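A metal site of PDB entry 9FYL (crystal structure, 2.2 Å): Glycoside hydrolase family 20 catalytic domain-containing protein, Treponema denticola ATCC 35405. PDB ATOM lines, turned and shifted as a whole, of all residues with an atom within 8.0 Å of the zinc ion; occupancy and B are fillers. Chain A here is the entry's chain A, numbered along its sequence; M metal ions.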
ATOM      1  N   LEU A  86       3.685 -17.106  31.267  1.00  0.00           N
ATOM      2  CA  LEU A  86       3.195 -17.390  29.925  1.00  0.00           C
ATOM      3  C   LEU A  86       1.869 -16.704  29.633  1.00  0.00           C
ATOM      4  O   LEU A  86       1.779 -15.827  28.758  1.00  0.00           O
ATOM      5  CB  LEU A  86       3.050 -18.896  29.725  1.00  0.00           C
ATOM      6  CG  LEU A  86       2.661 -19.403  28.330  1.00  0.00           C
ATOM      7  CD1 LEU A  86       3.469 -18.709  27.242  1.00  0.00           C
ATOM      8  CD2 LEU A  86       2.814 -20.918  28.255  1.00  0.00           C
ATOM      9  N   GLU A 104       7.205  -6.990  20.569  1.00  0.00           N
ATOM     10  CA  GLU A 104       7.587  -8.052  19.654  1.00  0.00           C
ATOM     11  C   GLU A 104       7.370  -9.441  20.253  1.00  0.00           C
ATOM     12  O   GLU A 104       7.275 -10.420  19.502  1.00  0.00           O
ATOM     13  CB  GLU A 104       9.057  -7.890  19.243  1.00  0.00           C
ATOM     14  CG  GLU A 104      10.033  -7.933  20.424  1.00  0.00           C
ATOM     15  CD  GLU A 104      10.392  -6.556  20.978  1.00  0.00           C
ATOM     16  OE1 GLU A 104       9.472  -5.741  21.212  1.00  0.00           O
ATOM     17  OE2 GLU A 104      11.597  -6.311  21.192  1.00  0.00           O
ATOM     18  N   LEU A 105       7.280  -9.549  21.575  1.00  0.00           N
ATOM     19  CA  LEU A 105       7.159 -10.831  22.246  1.00  0.00           C
ATOM     20  C   LEU A 105       5.714 -11.257  22.467  1.00  0.00           C
ATOM     21  O   LEU A 105       5.479 -12.290  23.117  1.00  0.00           O
ATOM     22  CB  LEU A 105       7.903 -10.786  23.587  1.00  0.00           C
ATOM     23  CG  LEU A 105       9.369 -10.339  23.538  1.00  0.00           C
ATOM     24  CD1 LEU A 105      10.040 -10.426  24.904  1.00  0.00           C
ATOM     25  CD2 LEU A 105      10.141 -11.150  22.506  1.00  0.00           C
ATOM     26  N   ASP A 106       4.758 -10.486  21.963  1.00  0.00           N
ATOM     27  CA  ASP A 106       3.356 -10.854  22.037  1.00  0.00           C
ATOM     28  C   ASP A 106       3.100 -12.077  21.163  1.00  0.00           C
ATOM     29  O   ASP A 106       3.629 -12.184  20.046  1.00  0.00           O
ATOM     30  CB  ASP A 106       2.496  -9.672  21.575  1.00  0.00           C
ATOM     31  CG  ASP A 106       1.006  -9.908  21.764  1.00  0.00           C
ATOM     32  OD1 ASP A 106       0.595 -10.693  22.643  1.00  0.00           O
ATOM     33  OD2 ASP A 106       0.244  -9.268  21.017  1.00  0.00           O
ATOM     34  N   GLU A 107       2.305 -13.011  21.677  1.00  0.00           N
ATOM     35  CA  GLU A 107       1.948 -14.188  20.888  1.00  0.00           C
ATOM     36  C   GLU A 107       0.966 -13.855  19.765  1.00  0.00           C
ATOM     37  O   GLU A 107       0.888 -14.592  18.782  1.00  0.00           O
ATOM     38  CB  GLU A 107       1.328 -15.259  21.785  1.00  0.00           C
ATOM     39  CG  GLU A 107       0.757 -16.463  21.042  1.00  0.00           C
ATOM     40  CD  GLU A 107       1.834 -17.339  20.440  1.00  0.00           C
ATOM     41  OE1 GLU A 107       3.018 -16.952  20.469  1.00  0.00           O
ATOM     42  OE2 GLU A 107       1.487 -18.437  19.930  1.00  0.00           O
ATOM     43  N   THR A 108       0.208 -12.773  19.901  1.00  0.00           N
ATOM     44  CA  THR A 108      -0.839 -12.402  18.941  1.00  0.00           C
ATOM     45  C   THR A 108      -0.583 -10.984  18.441  1.00  0.00           C
ATOM     46  O   THR A 108      -1.408 -10.091  18.644  1.00  0.00           O
ATOM     47  CB  THR A 108      -2.213 -12.521  19.577  1.00  0.00           C
ATOM     48  OG1 THR A 108      -2.360 -11.497  20.579  1.00  0.00           O
ATOM     49  CG2 THR A 108      -2.384 -13.877  20.222  1.00  0.00           C
ATOM     50  N   PRO A 109       0.554 -10.743  17.796  1.00  0.00           N
ATOM     51  CA  PRO A 109       0.882  -9.371  17.407  1.00  0.00           C
ATOM     52  C   PRO A 109      -0.198  -8.770  16.522  1.00  0.00           C
ATOM     53  O   PRO A 109      -0.640  -9.389  15.550  1.00  0.00           O
ATOM     54  CB  PRO A 109       2.222  -9.518  16.663  1.00  0.00           C
ATOM     55  CG  PRO A 109       2.392 -11.003  16.399  1.00  0.00           C
ATOM     56  CD  PRO A 109       1.645 -11.689  17.503  1.00  0.00           C
ATOM     57  N   SER A 122      -0.854 -13.484  26.021  1.00  0.00           N
ATOM     58  CA  SER A 122       0.221 -14.351  26.481  1.00  0.00           C
ATOM     59  C   SER A 122       1.504 -14.026  25.736  1.00  0.00           C
ATOM     60  O   SER A 122       1.493 -13.421  24.654  1.00  0.00           O
ATOM     61  CB  SER A 122      -0.135 -15.843  26.309  1.00  0.00           C
ATOM     62  OG  SER A 122      -0.573 -16.110  25.002  1.00  0.00           O
ATOM     63  N   LEU A 123       2.612 -14.411  26.341  1.00  0.00           N
ATOM     64  CA  LEU A 123       3.909 -14.288  25.719  1.00  0.00           C
ATOM     65  C   LEU A 123       4.105 -15.371  24.662  1.00  0.00           C
ATOM     66  O   LEU A 123       3.494 -16.440  24.726  1.00  0.00           O
ATOM     67  CB  LEU A 123       5.011 -14.412  26.767  1.00  0.00           C
ATOM     68  CG  LEU A 123       4.888 -13.507  27.992  1.00  0.00           C
ATOM     69  CD1 LEU A 123       5.991 -13.878  28.975  1.00  0.00           C
ATOM     70  CD2 LEU A 123       4.975 -12.050  27.573  1.00  0.00           C
ATOM     71  N   CYS A 124       4.953 -15.076  23.680  1.00  0.00           N
ATOM     72  CA  CYS A 124       5.331 -16.092  22.700  1.00  0.00           C
ATOM     73  C   CYS A 124       6.267 -17.102  23.361  1.00  0.00           C
ATOM     74  O   CYS A 124       7.376 -16.747  23.784  1.00  0.00           O
ATOM     75  CB  CYS A 124       6.007 -15.453  21.489  1.00  0.00           C
ATOM     76  SG  CYS A 124       6.626 -16.668  20.293  1.00  0.00           S
ATOM     77  N   SER A 125       5.821 -18.354  23.450  1.00  0.00           N
ATOM     78  CA  SER A 125       6.613 -19.379  24.140  1.00  0.00           C
ATOM     79  C   SER A 125       7.812 -19.854  23.327  1.00  0.00           C
ATOM     80  O   SER A 125       8.647 -20.601  23.866  1.00  0.00           O
ATOM     81  CB  SER A 125       5.749 -20.585  24.488  1.00  0.00           C
ATOM     82  OG  SER A 125       5.331 -21.255  23.300  1.00  0.00           O
ATOM     83  N   SER A 126       7.941 -19.434  22.069  1.00  0.00           N
ATOM     84  CA  SER A 126       9.039 -19.863  21.218  1.00  0.00           C
ATOM     85  C   SER A 126      10.134 -18.809  21.090  1.00  0.00           C
ATOM     86  O   SER A 126      11.177 -19.089  20.483  1.00  0.00           O
ATOM     87  CB  SER A 126       8.517 -20.217  19.819  1.00  0.00           C
ATOM     88  OG  SER A 126       7.830 -21.459  19.806  1.00  0.00           O
ATOM     89  N   ASN A 127       9.914 -17.611  21.598  1.00  0.00           N
ATOM     90  CA  ASN A 127      10.830 -16.494  21.429  1.00  0.00           C
ATOM     91  C   ASN A 127      11.844 -16.509  22.569  1.00  0.00           C
ATOM     92  O   ASN A 127      11.474 -16.362  23.737  1.00  0.00           O
ATOM     93  CB  ASN A 127      10.088 -15.167  21.396  1.00  0.00           C
ATOM     94  CG  ASN A 127      10.952 -14.018  20.917  1.00  0.00           C
ATOM     95  OD1 ASN A 127      12.096 -13.852  21.367  1.00  0.00           O
ATOM     96  ND2 ASN A 127      10.433 -13.219  19.992  1.00  0.00           N
ATOM     97  N   LEU A 159      -4.067 -18.506  24.539  1.00  0.00           N
ATOM     98  CA  LEU A 159      -3.404 -18.058  23.321  1.00  0.00           C
ATOM     99  C   LEU A 159      -2.026 -18.700  23.263  1.00  0.00           C
ATOM    100  O   LEU A 159      -1.120 -18.329  24.027  1.00  0.00           O
ATOM    101  CB  LEU A 159      -3.328 -16.536  23.278  1.00  0.00           C
ATOM    102  CG  LEU A 159      -4.671 -15.808  23.167  1.00  0.00           C
ATOM    103  CD1 LEU A 159      -4.471 -14.315  23.390  1.00  0.00           C
ATOM    104  CD2 LEU A 159      -5.329 -16.078  21.819  1.00  0.00           C
ATOM    105  N   ILE A 160      -1.856 -19.657  22.355  1.00  0.00           N
ATOM    106  CA  ILE A 160      -0.632 -20.425  22.243  1.00  0.00           C
ATOM    107  C   ILE A 160      -0.714 -21.166  20.917  1.00  0.00           C
ATOM    108  O   ILE A 160      -1.738 -21.782  20.606  1.00  0.00           O
ATOM    109  CB  ILE A 160      -0.462 -21.379  23.433  1.00  0.00           C
ATOM    110  CG1 ILE A 160       0.808 -22.220  23.266  1.00  0.00           C
ATOM    111  CG2 ILE A 160      -1.694 -22.264  23.586  1.00  0.00           C
ATOM    112  CD1 ILE A 160       1.151 -23.045  24.478  1.00  0.00           C
ATOM    113  N   GLY A 161       0.344 -21.095  20.119  1.00  0.00           N
ATOM    114  CA  GLY A 161       0.272 -21.624  18.772  1.00  0.00           C
ATOM    115  C   GLY A 161      -0.707 -20.893  17.894  1.00  0.00           C
ATOM    116  O   GLY A 161      -1.344 -21.509  17.041  1.00  0.00           O
ATOM    117  N   GLU A 162      -0.835 -19.589  18.074  1.00  0.00           N
ATOM    118  CA  GLU A 162      -1.831 -18.803  17.358  1.00  0.00           C
ATOM    119  C   GLU A 162      -1.348 -18.500  15.945  1.00  0.00           C
ATOM    120  O   GLU A 162      -0.142 -18.382  15.687  1.00  0.00           O
ATOM    121  CB  GLU A 162      -2.121 -17.511  18.108  1.00  0.00           C
ATOM    122  CG  GLU A 162      -2.678 -17.734  19.503  1.00  0.00           C
ATOM    123  CD  GLU A 162      -3.924 -18.599  19.483  1.00  0.00           C
ATOM    124  OE1 GLU A 162      -4.830 -18.301  18.667  1.00  0.00           O
ATOM    125  OE2 GLU A 162      -4.004 -19.581  20.253  1.00  0.00           O
ATOM    126  N   ALA A 164      -1.454 -15.828  14.339  1.00  0.00           N
ATOM    127  CA  ALA A 164      -0.792 -14.534  14.201  1.00  0.00           C
ATOM    128  C   ALA A 164       0.693 -14.589  14.542  1.00  0.00           C
ATOM    129  O   ALA A 164       1.427 -13.676  14.151  1.00  0.00           O
ATOM    130  CB  ALA A 164      -1.494 -13.490  15.088  1.00  0.00           C
ATOM    131  N   CYS A 165       1.154 -15.606  15.267  1.00  0.00           N
ATOM    132  CA  CYS A 165       2.560 -15.676  15.665  1.00  0.00           C
ATOM    133  C   CYS A 165       3.386 -16.279  14.531  1.00  0.00           C
ATOM    134  O   CYS A 165       3.135 -17.413  14.112  1.00  0.00           O
ATOM    135  CB  CYS A 165       2.684 -16.514  16.936  1.00  0.00           C
ATOM    136  SG  CYS A 165       4.365 -16.598  17.577  1.00  0.00           S
ATOM    137  N   PRO A 166       4.406 -15.565  14.030  1.00  0.00           N
ATOM    138  CA  PRO A 166       5.226 -16.096  12.900  1.00  0.00           C
ATOM    139  C   PRO A 166       6.042 -17.305  13.292  1.00  0.00           C
ATOM    140  O   PRO A 166       6.572 -18.028  12.417  1.00  0.00           O
ATOM    141  CB  PRO A 166       6.139 -14.918  12.542  1.00  0.00           C
ATOM    142  CG  PRO A 166       5.874 -13.807  13.565  1.00  0.00           C
ATOM    143  CD  PRO A 166       4.847 -14.251  14.532  1.00  0.00           C
ATOM    144  N   LEU A 167       6.175 -17.470  14.598  1.00  0.00           N
ATOM    145  CA  LEU A 167       6.997 -18.342  15.424  1.00  0.00           C
ATOM    146  C   LEU A 167       6.328 -19.626  15.841  1.00  0.00           C
ATOM    147  O   LEU A 167       6.956 -20.683  15.858  1.00  0.00           O
ATOM    148  CB  LEU A 167       7.351 -17.522  16.728  1.00  0.00           C
ATOM    149  CG  LEU A 167       8.670 -16.863  17.197  1.00  0.00           C
ATOM    150  CD1 LEU A 167       9.881 -17.449  18.015  1.00  0.00           C
ATOM    151  CD2 LEU A 167       8.901 -16.509  15.361  1.00  0.00           C
ATOM    152  N   CYS A 168       5.045 -19.521  16.231  1.00  0.00           N
ATOM    153  CA  CYS A 168       4.311 -20.656  16.747  1.00  0.00           C
ATOM    154  C   CYS A 168       3.197 -21.130  15.824  1.00  0.00           C
ATOM    155  O   CYS A 168       2.607 -22.191  16.078  1.00  0.00           O
ATOM    156  CB  CYS A 168       3.692 -20.330  18.120  1.00  0.00           C
ATOM    157  SG  CYS A 168       4.871 -19.829  19.401  1.00  0.00           S
ATOM    158  N   ARG A 169       2.876 -20.385  14.764  1.00  0.00           N
ATOM    159  CA  ARG A 169       1.726 -20.742  13.945  1.00  0.00           C
ATOM    160  C   ARG A 169       1.847 -22.172  13.410  1.00  0.00           C
ATOM    161  O   ARG A 169       2.902 -22.562  12.905  1.00  0.00           O
ATOM    162  CB  ARG A 169       1.551 -19.763  12.789  1.00  0.00           C
ATOM    163  CG  ARG A 169       2.570 -19.897  11.679  1.00  0.00           C
ATOM    164  CD  ARG A 169       2.385 -18.833  10.614  1.00  0.00           C
ATOM    165  NE  ARG A 169       2.139 -17.514  11.190  1.00  0.00           N
ATOM    166  CZ  ARG A 169       2.468 -16.367  10.618  1.00  0.00           C
ATOM    167  NH1 ARG A 169       3.079 -16.338   9.440  1.00  0.00           N
ATOM    168  NH2 ARG A 169       2.176 -15.225  11.223  1.00  0.00           N
ATOM    169  N   LYS A 171       1.982 -24.986  14.961  1.00  0.00           N
ATOM    170  CA  LYS A 171       2.636 -25.942  15.825  1.00  0.00           C
ATOM    171  C   LYS A 171       1.647 -26.525  16.823  1.00  0.00           C
ATOM    172  O   LYS A 171       0.551 -25.996  17.036  1.00  0.00           O
ATOM    173  CB  LYS A 171       3.790 -25.268  16.567  1.00  0.00           C
ATOM    174  CG  LYS A 171       4.734 -24.496  15.659  1.00  0.00           C
ATOM    175  CD  LYS A 171       6.069 -25.182  15.468  1.00  0.00           C
ATOM    176  CE  LYS A 171       7.087 -24.185  14.915  1.00  0.00           C
ATOM    177  NZ  LYS A 171       8.394 -24.275  15.626  1.00  0.00           N
ATOM    178  N   LEU A 176       4.143 -27.130  22.396  1.00  0.00           N
ATOM    179  CA  LEU A 176       4.561 -25.772  22.741  1.00  0.00           C
ATOM    180  C   LEU A 176       4.484 -25.543  24.240  1.00  0.00           C
ATOM    181  O   LEU A 176       5.430 -25.036  24.854  1.00  0.00           O
ATOM    182  CB  LEU A 176       3.702 -24.748  22.007  1.00  0.00           C
ATOM    183  CG  LEU A 176       3.977 -24.544  20.515  1.00  0.00           C
ATOM    184  CD1 LEU A 176       2.725 -23.980  19.849  1.00  0.00           C
ATOM    185  CD2 LEU A 176       5.158 -23.613  20.296  1.00  0.00           C
HETATM  186 ZN    ZN M   1       4.577 -17.639  19.492  1.00  0.00          ZN
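Leu 167 touches the zinc ion (CB to ZN, 3.9 Å). The nearest printed residue that does not touch the zinc ion is Ser 125 (4.2 Å).
The backbone carbonyl oxygen (O) of Ser 122 is in hydrogen-bond range of the backbone NH (N) of Glu 107 (3.1 Å). N of Asn 127 lies close to SG of Cys 124, 3.7 Å away. The backbone carbonyl oxygen of Leu 105 sits at hydrogen-bond distance from the backbone NH of Cys 124, at 2.9 Å. The side-chain sulfur (SG) of Cys 168 lies close to the side-chain hydroxyl (OG) of Ser 126. The side-chain sulfur (SG) of Cys 124 lies close to the backbone NH (N) of Ser 126 (3.5 Å). The side-chain carboxylate (OE2) of Glu 107 sits at hydrogen-bond distance from the backbone NH (N) of Gly 161 (2.9 Å). NE of Arg 169 sits at hydrogen-bond distance from O of Cys 165 (3.1 Å). OE2 of Glu 107 lies within hydrogen-bond range of N of Glu 162, at 3.2 Å.
OE1 of Glu 107 binds the zinc ion (2.0 Å). SG of Cys 165 binds the zinc ion (2.2 Å). SG of Cys 168 binds the zinc ion (2.2 Å). The side-chain sulfur (SG) of Cys 124 is bound to the zinc ion, 2.4 Å away.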
